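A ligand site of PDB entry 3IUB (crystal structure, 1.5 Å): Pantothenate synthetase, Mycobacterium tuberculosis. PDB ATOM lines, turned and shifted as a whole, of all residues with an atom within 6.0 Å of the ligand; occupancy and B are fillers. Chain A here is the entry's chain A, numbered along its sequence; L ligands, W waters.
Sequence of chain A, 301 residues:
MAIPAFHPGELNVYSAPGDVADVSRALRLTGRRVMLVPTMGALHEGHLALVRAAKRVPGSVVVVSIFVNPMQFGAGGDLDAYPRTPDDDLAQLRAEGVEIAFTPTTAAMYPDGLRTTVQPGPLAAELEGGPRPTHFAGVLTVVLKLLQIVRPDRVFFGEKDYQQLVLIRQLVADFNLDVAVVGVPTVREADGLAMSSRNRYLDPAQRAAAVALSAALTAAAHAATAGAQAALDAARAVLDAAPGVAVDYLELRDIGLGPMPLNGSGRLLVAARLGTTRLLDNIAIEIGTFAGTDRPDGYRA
A ring nitrogen (NE2) of His 47 lies within hydrogen-bond range of an oxygen (O3) of the ligand. The backbone NH of Val 187 lies within hydrogen-bond range of an oxygen (O4) of the ligand, 3.0 Å away. The backbone NH of Met 40 sits at hydrogen-bond distance from an oxygen (O3) of the ligand. N1 of the ligand sits at hydrogen-bond distance from NE2 of Gln 164.
OG1 of Thr 186 sits at hydrogen-bond distance from N of Lys 160 (3.2 Å). A ring nitrogen (NE2) of His 44 lies close to the backbone NH (N) of Ser 197 (3.5 Å). The side-chain hydroxyl (OG1) of Thr 39 is in hydrogen-bond range of the backbone NH (N) of Gly 41 (3.1 Å). The side-chain sulfur of Met 40 lies close to the side-chain amide oxygen of Gln 72 (3.6 Å). The backbone carbonyl oxygen (O) of Phe 157 sits at hydrogen-bond distance from the backbone NH (N) of Val 184 (2.8 Å). The backbone carbonyl oxygen (O) of Met 195 sits at hydrogen-bond distance from the side-chain amino group (NZ) of Lys 160, 3.1 Å away. The backbone carbonyl oxygen (O) of Val 187 lies within hydrogen-bond range of the backbone NH (N) of Met 195. O of Val 184 lies within hydrogen-bond range of N of Glu 159 (2.9 Å).
O of Pro 38 lies close to O2 of the ligand. Merely in contact with the ligand: Pro 185 (3.2 Å), Met 195 (3.2 Å), Gly 46 (3.3 Å), Tyr 82 (3.4 Å), His 44 (3.5 Å), Thr 186 (3.6 Å), Thr 39 (3.6 Å), Asp 161 (3.6 Å), Lys 160 (3.7 Å), Val 184 (3.7 Å), Leu 50 (3.8 Å), Gly 158 (3.8 Å) and Ala 49 (3.9 Å). Within 4 Å of the ligand: Pro 38, Thr 39, Met 40, His 44, Gly 46, His 47, Ala 49, Leu 50, Tyr 82, Gly 158, Lys 160, Asp 161, Gln 164, Val 184, Pro 185, Thr 186, Val 187 and Met 195. The nearest printed residue that does not touch the ligand is Gln 72 (4.6 Å).
Water W1 lies within hydrogen-bond range of N of Glu 159 (2.7 Å), O4 of the ligand (2.8 Å), N of Lys 160 (3.0 Å), O of Val 184 (3.1 Å) and OG1 of Thr 186 (3.5 Å). Water W4 bridges the side-chain carboxylate of Asp 161 (2.5 Å) and an oxygen (O1) of the ligand (3.1 Å). Water W5 lies within hydrogen-bond range of the backbone NH of Gly 158 (2.9 Å) and a nitrogen (N2) of the ligand (3.2 Å). Water W3 lies within hydrogen-bond range of the side-chain hydroxyl of Tyr 82 (2.6 Å), the backbone carbonyl oxygen of Gly 41 (2.7 Å), the side-chain hydroxyl of Ser 197 (2.9 Å) and an oxygen (O3) of the ligand (3.4 Å).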
ATOM      1  N   PRO A  38       3.192  14.318  -2.223  1.00  0.00           N
ATOM      2  CA  PRO A  38       4.018  14.720  -3.376  1.00  0.00           C
ATOM      3  C   PRO A  38       5.485  14.599  -3.049  1.00  0.00           C
ATOM      4  O   PRO A  38       5.955  15.111  -2.040  1.00  0.00           O
ATOM      5  CB  PRO A  38       3.654  16.193  -3.598  1.00  0.00           C
ATOM      6  CG  PRO A  38       2.674  16.560  -2.530  1.00  0.00           C
ATOM      7  CD  PRO A  38       2.711  15.489  -1.474  1.00  0.00           C
ATOM      8  N   THR A  39       6.220  13.914  -3.920  1.00  0.00           N
ATOM      9  CA  THR A  39       7.632  13.685  -3.695  1.00  0.00           C
ATOM     10  C   THR A  39       8.422  13.894  -4.979  1.00  0.00           C
ATOM     11  O   THR A  39       7.879  13.844  -6.075  1.00  0.00           O
ATOM     12  CB  THR A  39       7.949  12.229  -3.236  1.00  0.00           C
ATOM     13  OG1 THR A  39       7.931  11.333  -4.360  1.00  0.00           O
ATOM     14  CG2 THR A  39       6.964  11.710  -2.187  1.00  0.00           C
ATOM     15  N   MET A  40       9.731  14.066  -4.821  1.00  0.00           N
ATOM     16  CA  MET A  40      10.622  14.034  -5.975  1.00  0.00           C
ATOM     17  C   MET A  40      11.349  12.685  -6.111  1.00  0.00           C
ATOM     18  O   MET A  40      12.438  12.619  -6.670  1.00  0.00           O
ATOM     19  CB  MET A  40      11.606  15.195  -5.892  1.00  0.00           C
ATOM     20  CG  MET A  40      10.902  16.525  -5.827  1.00  0.00           C
ATOM     21  SD  MET A  40      11.601  17.754  -6.962  1.00  0.00           S
ATOM     22  CE  MET A  40      13.202  18.044  -6.204  1.00  0.00           C
ATOM     23  N   GLY A  41      10.714  11.616  -5.613  1.00  0.00           N
ATOM     24  CA  GLY A  41      11.313  10.272  -5.692  1.00  0.00           C
ATOM     25  C   GLY A  41      12.521  10.136  -4.785  1.00  0.00           C
ATOM     26  O   GLY A  41      12.700  10.903  -3.824  1.00  0.00           O
ATOM     27  N   HIS A  44      12.895   7.683   0.880  1.00  0.00           N
ATOM     28  CA  HIS A  44      13.510   7.197   2.102  1.00  0.00           C
ATOM     29  C   HIS A  44      12.467   7.172   3.219  1.00  0.00           C
ATOM     30  O   HIS A  44      11.295   7.499   3.006  1.00  0.00           O
ATOM     31  CB  HIS A  44      14.708   8.076   2.475  1.00  0.00           C
ATOM     32  CG  HIS A  44      14.394   9.535   2.501  1.00  0.00           C
ATOM     33  ND1 HIS A  44      13.570  10.105   3.437  1.00  0.00           N
ATOM     34  CD2 HIS A  44      14.806  10.545   1.695  1.00  0.00           C
ATOM     35  CE1 HIS A  44      13.469  11.401   3.202  1.00  0.00           C
ATOM     36  NE2 HIS A  44      14.223  11.695   2.155  1.00  0.00           N
ATOM     37  N   GLU A  45      12.891   6.819   4.435  1.00  0.00           N
ATOM     38  CA  GLU A  45      11.955   6.607   5.542  1.00  0.00           C
ATOM     39  C   GLU A  45      11.141   7.847   5.903  1.00  0.00           C
ATOM     40  O   GLU A  45      10.037   7.745   6.457  1.00  0.00           O
ATOM     41  CB  GLU A  45      12.701   6.120   6.775  1.00  0.00           C
ATOM     42  CG  GLU A  45      12.939   4.620   6.782  1.00  0.00           C
ATOM     43  CD  GLU A  45      11.655   3.837   6.916  1.00  0.00           C
ATOM     44  OE1 GLU A  45      11.440   2.927   6.080  1.00  0.00           O
ATOM     45  OE2 GLU A  45      10.865   4.114   7.850  1.00  0.00           O
ATOM     46  N   GLY A  46      11.706   9.013   5.602  1.00  0.00           N
ATOM     47  CA  GLY A  46      10.993  10.278   5.780  1.00  0.00           C
ATOM     48  C   GLY A  46       9.751  10.329   4.896  1.00  0.00           C
ATOM     49  O   GLY A  46       8.648  10.650   5.356  1.00  0.00           O
ATOM     50  N   HIS A  47       9.932  10.005   3.612  1.00  0.00           N
ATOM     51  CA  HIS A  47       8.793   9.909   2.703  1.00  0.00           C
ATOM     52  C   HIS A  47       7.812   8.845   3.188  1.00  0.00           C
ATOM     53  O   HIS A  47       6.595   9.041   3.119  1.00  0.00           O
ATOM     54  CB  HIS A  47       9.217   9.561   1.282  1.00  0.00           C
ATOM     55  CG  HIS A  47      10.119  10.558   0.640  1.00  0.00           C
ATOM     56  ND1 HIS A  47      11.460  10.333   0.463  1.00  0.00           N
ATOM     57  CD2 HIS A  47       9.874  11.787   0.101  1.00  0.00           C
ATOM     58  CE1 HIS A  47      12.008  11.358  -0.147  1.00  0.00           C
ATOM     59  NE2 HIS A  47      11.067  12.246  -0.389  1.00  0.00           N
ATOM     60  N   ALA A  49       7.201   7.846   6.243  1.00  0.00           N
ATOM     61  CA  ALA A  49       6.438   8.422   7.364  1.00  0.00           C
ATOM     62  C   ALA A  49       5.260   9.248   6.841  1.00  0.00           C
ATOM     63  O   ALA A  49       4.187   9.227   7.450  1.00  0.00           O
ATOM     64  CB  ALA A  49       7.341   9.273   8.233  1.00  0.00           C
ATOM     65  N   LEU A  50       5.437   9.952   5.725  1.00  0.00           N
ATOM     66  CA  LEU A  50       4.305  10.682   5.138  1.00  0.00           C
ATOM     67  C   LEU A  50       3.225   9.719   4.658  1.00  0.00           C
ATOM     68  O   LEU A  50       2.031   9.931   4.904  1.00  0.00           O
ATOM     69  CB  LEU A  50       4.763  11.546   3.966  1.00  0.00           C
ATOM     70  CG  LEU A  50       5.908  12.536   4.197  1.00  0.00           C
ATOM     71  CD1 LEU A  50       6.125  13.370   2.961  1.00  0.00           C
ATOM     72  CD2 LEU A  50       5.677  13.433   5.406  1.00  0.00           C
ATOM     73  N   GLN A  72      11.983  23.898 -10.435  1.00  0.00           N
ATOM     74  CA  GLN A  72      12.520  24.354  -9.156  1.00  0.00           C
ATOM     75  C   GLN A  72      14.035  24.217  -9.111  1.00  0.00           C
ATOM     76  O   GLN A  72      14.642  24.350  -8.049  1.00  0.00           O
ATOM     77  CB  GLN A  72      11.848  23.630  -7.990  1.00  0.00           C
ATOM     78  CG  GLN A  72      12.111  22.123  -7.882  1.00  0.00           C
ATOM     79  CD  GLN A  72      11.269  21.486  -6.782  1.00  0.00           C
ATOM     80  OE1 GLN A  72      11.781  21.132  -5.698  1.00  0.00           O
ATOM     81  NE2 GLN A  72       9.975  21.371  -7.036  1.00  0.00           N
ATOM     82  N   TYR A  82      20.145  15.178  -9.582  1.00  0.00           N
ATOM     83  CA  TYR A  82      19.208  14.720  -8.571  1.00  0.00           C
ATOM     84  C   TYR A  82      19.081  13.206  -8.591  1.00  0.00           C
ATOM     85  O   TYR A  82      18.946  12.626  -9.674  1.00  0.00           O
ATOM     86  CB  TYR A  82      17.822  15.365  -8.743  1.00  0.00           C
ATOM     87  CG  TYR A  82      17.062  15.349  -7.450  1.00  0.00           C
ATOM     88  CD1 TYR A  82      17.323  16.296  -6.458  1.00  0.00           C
ATOM     89  CD2 TYR A  82      16.120  14.347  -7.181  1.00  0.00           C
ATOM     90  CE1 TYR A  82      16.659  16.270  -5.224  1.00  0.00           C
ATOM     91  CE2 TYR A  82      15.435  14.318  -5.952  1.00  0.00           C
ATOM     92  CZ  TYR A  82      15.715  15.285  -4.992  1.00  0.00           C
ATOM     93  OH  TYR A  82      15.047  15.256  -3.781  1.00  0.00           O
ATOM     94  N   HIS A 135      13.313  29.415  -7.060  1.00  0.00           N
ATOM     95  CA  HIS A 135      13.188  28.048  -6.548  1.00  0.00           C
ATOM     96  C   HIS A 135      11.772  27.779  -6.032  1.00  0.00           C
ATOM     97  O   HIS A 135      11.127  26.811  -6.437  1.00  0.00           O
ATOM     98  CB  HIS A 135      14.187  27.753  -5.407  1.00  0.00           C
ATOM     99  CG  HIS A 135      13.890  26.456  -4.708  1.00  0.00           C
ATOM    100  ND1 HIS A 135      14.129  25.226  -5.284  1.00  0.00           N
ATOM    101  CD2 HIS A 135      13.333  26.195  -3.502  1.00  0.00           C
ATOM    102  CE1 HIS A 135      13.752  24.264  -4.448  1.00  0.00           C
ATOM    103  NE2 HIS A 135      13.260  24.834  -3.368  1.00  0.00           N
ATOM    104  N   PHE A 157       3.295  16.853   3.857  1.00  0.00           N
ATOM    105  CA  PHE A 157       4.687  17.317   3.684  1.00  0.00           C
ATOM    106  C   PHE A 157       5.503  17.086   4.948  1.00  0.00           C
ATOM    107  O   PHE A 157       4.971  17.096   6.060  1.00  0.00           O
ATOM    108  CB  PHE A 157       4.705  18.805   3.326  1.00  0.00           C
ATOM    109  CG  PHE A 157       4.217  19.100   1.940  1.00  0.00           C
ATOM    110  CD1 PHE A 157       5.078  18.967   0.847  1.00  0.00           C
ATOM    111  CD2 PHE A 157       2.880  19.475   1.723  1.00  0.00           C
ATOM    112  CE1 PHE A 157       4.610  19.219  -0.461  1.00  0.00           C
ATOM    113  CE2 PHE A 157       2.423  19.722   0.455  1.00  0.00           C
ATOM    114  CZ  PHE A 157       3.269  19.598  -0.641  1.00  0.00           C
ATOM    115  N   GLY A 158       6.814  16.889   4.769  1.00  0.00           N
ATOM    116  CA  GLY A 158       7.701  16.793   5.915  1.00  0.00           C
ATOM    117  C   GLY A 158       8.002  18.157   6.505  1.00  0.00           C
ATOM    118  O   GLY A 158       8.011  19.163   5.803  1.00  0.00           O
ATOM    119  N   GLU A 159       8.276  18.191   7.811  1.00  0.00           N
ATOM    120  CA  GLU A 159       8.722  19.428   8.448  1.00  0.00           C
ATOM    121  C   GLU A 159      10.194  19.689   8.168  1.00  0.00           C
ATOM    122  O   GLU A 159      10.697  20.747   8.488  1.00  0.00           O
ATOM    123  CB  GLU A 159       8.524  19.385   9.965  1.00  0.00           C
ATOM    124  CG  GLU A 159       7.060  19.473  10.414  1.00  0.00           C
ATOM    125  CD  GLU A 159       6.884  19.595  11.921  1.00  0.00           C
ATOM    126  OE1 GLU A 159       7.846  19.422  12.684  1.00  0.00           O
ATOM    127  OE2 GLU A 159       5.737  19.878  12.325  1.00  0.00           O
ATOM    128  N   LYS A 160      10.881  18.726   7.565  1.00  0.00           N
ATOM    129  CA  LYS A 160      12.311  18.876   7.289  1.00  0.00           C
ATOM    130  C   LYS A 160      12.534  20.092   6.392  1.00  0.00           C
ATOM    131  O   LYS A 160      13.387  20.947   6.671  1.00  0.00           O
ATOM    132  CB  LYS A 160      12.844  17.597   6.626  1.00  0.00           C
ATOM    133  CG  LYS A 160      14.360  17.532   6.440  1.00  0.00           C
ATOM    134  CD  LYS A 160      14.801  18.333   5.204  1.00  0.00           C
ATOM    135  CE  LYS A 160      16.129  17.859   4.685  1.00  0.00           C
ATOM    136  NZ  LYS A 160      16.745  16.945   5.671  1.00  0.00           N
ATOM    137  N   ASP A 161      11.743  20.173   5.320  1.00  0.00           N
ATOM    138  CA  ASP A 161      11.804  21.345   4.450  1.00  0.00           C
ATOM    139  C   ASP A 161      10.746  22.327   4.952  1.00  0.00           C
ATOM    140  O   ASP A 161       9.680  22.520   4.368  1.00  0.00           O
ATOM    141  CB  ASP A 161      11.593  20.946   2.990  1.00  0.00           C
ATOM    142  CG  ASP A 161      12.737  20.089   2.474  1.00  0.00           C
ATOM    143  OD1 ASP A 161      13.759  20.680   2.061  1.00  0.00           O
ATOM    144  OD2 ASP A 161      12.610  18.857   2.497  1.00  0.00           O
ATOM    145  N   GLN A 164       9.635  25.382   2.867  1.00  0.00           N
ATOM    146  CA  GLN A 164       8.723  24.898   1.829  1.00  0.00           C
ATOM    147  C   GLN A 164       7.297  24.655   2.382  1.00  0.00           C
ATOM    148  O   GLN A 164       6.295  25.068   1.761  1.00  0.00           O
ATOM    149  CB  GLN A 164       9.281  23.596   1.250  1.00  0.00           C
ATOM    150  CG  GLN A 164       8.387  22.927   0.235  1.00  0.00           C
ATOM    151  CD  GLN A 164       9.054  21.706  -0.327  1.00  0.00           C
ATOM    152  OE1 GLN A 164       9.806  21.796  -1.273  1.00  0.00           O
ATOM    153  NE2 GLN A 164       8.812  20.565   0.301  1.00  0.00           N
ATOM    154  N   VAL A 184       4.355  16.685   8.784  1.00  0.00           N
ATOM    155  CA  VAL A 184       4.754  15.491   9.532  1.00  0.00           C
ATOM    156  C   VAL A 184       6.157  15.682  10.128  1.00  0.00           C
ATOM    157  O   VAL A 184       7.088  16.026   9.413  1.00  0.00           O
ATOM    158  CB  VAL A 184       4.726  14.252   8.616  1.00  0.00           C
ATOM    159  CG1 VAL A 184       5.167  13.011   9.387  1.00  0.00           C
ATOM    160  CG2 VAL A 184       3.324  14.034   8.031  1.00  0.00           C
ATOM    161  N   PRO A 185       6.313  15.484  11.452  1.00  0.00           N
ATOM    162  CA  PRO A 185       7.627  15.695  12.064  1.00  0.00           C
ATOM    163  C   PRO A 185       8.741  14.880  11.417  1.00  0.00           C
ATOM    164  O   PRO A 185       8.520  13.733  10.998  1.00  0.00           O
ATOM    165  CB  PRO A 185       7.417  15.300  13.538  1.00  0.00           C
ATOM    166  CG  PRO A 185       5.932  15.502  13.756  1.00  0.00           C
ATOM    167  CD  PRO A 185       5.304  15.083  12.454  1.00  0.00           C
ATOM    168  N   THR A 186       9.913  15.505  11.337  1.00  0.00           N
ATOM    169  CA  THR A 186      11.094  14.981  10.669  1.00  0.00           C
ATOM    170  C   THR A 186      11.542  13.633  11.238  1.00  0.00           C
ATOM    171  O   THR A 186      11.744  13.511  12.441  1.00  0.00           O
ATOM    172  CB  THR A 186      12.260  15.993  10.789  1.00  0.00           C
ATOM    173  OG1 THR A 186      11.857  17.247  10.201  1.00  0.00           O
ATOM    174  CG2 THR A 186      13.511  15.505  10.099  1.00  0.00           C
ATOM    175  N   VAL A 187      11.654  12.630  10.355  1.00  0.00           N
ATOM    176  CA  VAL A 187      12.246  11.339  10.694  1.00  0.00           C
ATOM    177  C   VAL A 187      13.763  11.501  10.720  1.00  0.00           C
ATOM    178  O   VAL A 187      14.333  12.155   9.856  1.00  0.00           O
ATOM    179  CB  VAL A 187      11.880  10.260   9.674  1.00  0.00           C
ATOM    180  CG1 VAL A 187      12.464   8.917  10.097  1.00  0.00           C
ATOM    181  CG2 VAL A 187      10.385  10.140   9.566  1.00  0.00           C
ATOM    182  N   ALA A 194      18.790  14.243  10.133  1.00  0.00           N
ATOM    183  CA  ALA A 194      17.516  14.266   9.442  1.00  0.00           C
ATOM    184  C   ALA A 194      17.585  13.453   8.152  1.00  0.00           C
ATOM    185  O   ALA A 194      18.579  13.532   7.457  1.00  0.00           O
ATOM    186  CB  ALA A 194      17.124  15.695   9.133  1.00  0.00           C
ATOM    187  N   MET A 195      16.545  12.658   7.882  1.00  0.00           N
ATOM    188  CA  MET A 195      16.445  11.925   6.613  1.00  0.00           C
ATOM    189  C   MET A 195      16.478  12.873   5.417  1.00  0.00           C
ATOM    190  O   MET A 195      15.863  13.939   5.438  1.00  0.00           O
ATOM    191  CB  MET A 195      15.154  11.087   6.548  1.00  0.00           C
ATOM    192  CG  MET A 195      15.088   9.964   7.552  1.00  0.00           C
ATOM    193  SD  MET A 195      16.474   8.809   7.422  1.00  0.00           S
ATOM    194  CE  MET A 195      15.951   7.498   8.566  1.00  0.00           C
ATOM    195  N   SER A 196      17.226  12.487   4.388  1.00  0.00           N
ATOM    196  CA  SER A 196      17.297  13.286   3.165  1.00  0.00           C
ATOM    197  C   SER A 196      17.813  12.400   2.054  1.00  0.00           C
ATOM    198  O   SER A 196      18.677  11.554   2.293  1.00  0.00           O
ATOM    199  CB  SER A 196      18.255  14.478   3.315  1.00  0.00           C
ATOM    200  OG  SER A 196      18.491  15.084   2.050  1.00  0.00           O
ATOM    201  N   SER A 197      17.308  12.635   0.842  1.00  0.00           N
ATOM    202  CA  SER A 197      17.830  11.982  -0.361  1.00  0.00           C
ATOM    203  C   SER A 197      19.268  12.433  -0.679  1.00  0.00           C
ATOM    204  O   SER A 197      19.931  11.825  -1.529  1.00  0.00           O
ATOM    205  CB  SER A 197      16.925  12.277  -1.558  1.00  0.00           C
ATOM    206  OG  SER A 197      15.615  11.746  -1.350  1.00  0.00           O
HETATM  207  C1  LIG L   1       8.545  12.997   7.869  1.00  0.00           C
HETATM  208  C2  LIG L   1      14.064  20.415  -1.802  1.00  0.00           C
HETATM  209  O1  LIG L   1      12.456  15.092   0.554  1.00  0.00           O
HETATM  210  O2  LIG L   1       8.931  16.352  -1.550  1.00  0.00           O
HETATM  211  O3  LIG L   1      10.686  14.652  -2.089  1.00  0.00           O
HETATM  212  C3  LIG L   1      13.564  18.068  -2.213  1.00  0.00           C
HETATM  213  C4  LIG L   1      12.685  16.979  -2.067  1.00  0.00           C
HETATM  214  C5  LIG L   1      11.980  13.689   6.733  1.00  0.00           C
HETATM  215  C6  LIG L   1      12.635  14.075   5.565  1.00  0.00           C
HETATM  216  C7  LIG L   1      12.015  19.445  -1.004  1.00  0.00           C
HETATM  217  C8  LIG L   1       9.905  13.712   5.482  1.00  0.00           C
HETATM  218  C9  LIG L   1      10.160  14.356   3.120  1.00  0.00           C
HETATM  219  N1  LIG L   1      11.156  18.352  -0.866  1.00  0.00           N
HETATM  220  N2  LIG L   1      10.226  15.369   0.460  1.00  0.00           N
HETATM  221  N3  LIG L   1      12.311  14.659   3.209  1.00  0.00           N
HETATM  222  O4  LIG L   1       9.982  13.114   7.861  1.00  0.00           O
HETATM  223  C10 LIG L   1      11.356  15.047   1.107  1.00  0.00           C
HETATM  224  C11 LIG L   1      13.218  19.307  -1.675  1.00  0.00           C
HETATM  225  C12 LIG L   1      10.596  13.502   6.696  1.00  0.00           C
HETATM  226  C13 LIG L   1      11.472  17.156  -1.388  1.00  0.00           C
HETATM  227  C14 LIG L   1      11.255  14.695   2.414  1.00  0.00           C
HETATM  228  C15 LIG L   1      10.576  14.096   4.375  1.00  0.00           C
HETATM  229  C16 LIG L   1      11.911  14.278   4.427  1.00  0.00           C
HETATM  230  S1  LIG L   1      10.319  15.816  -1.178  1.00  0.00           S
HETATM  231  O   HOH W   1       9.697  15.932   7.835  1.00  0.00           O
HETATM  232  O   HOH W   2      10.149  20.258  -3.494  1.00  0.00           O
HETATM  233  O   HOH W   3      13.664  13.251  -2.829  1.00  0.00           O
HETATM  234  O   HOH W   4      14.301  17.481   1.251  1.00  0.00           O
HETATM  235  O   HOH W   5       7.778  16.765   2.020  1.00  0.00           O
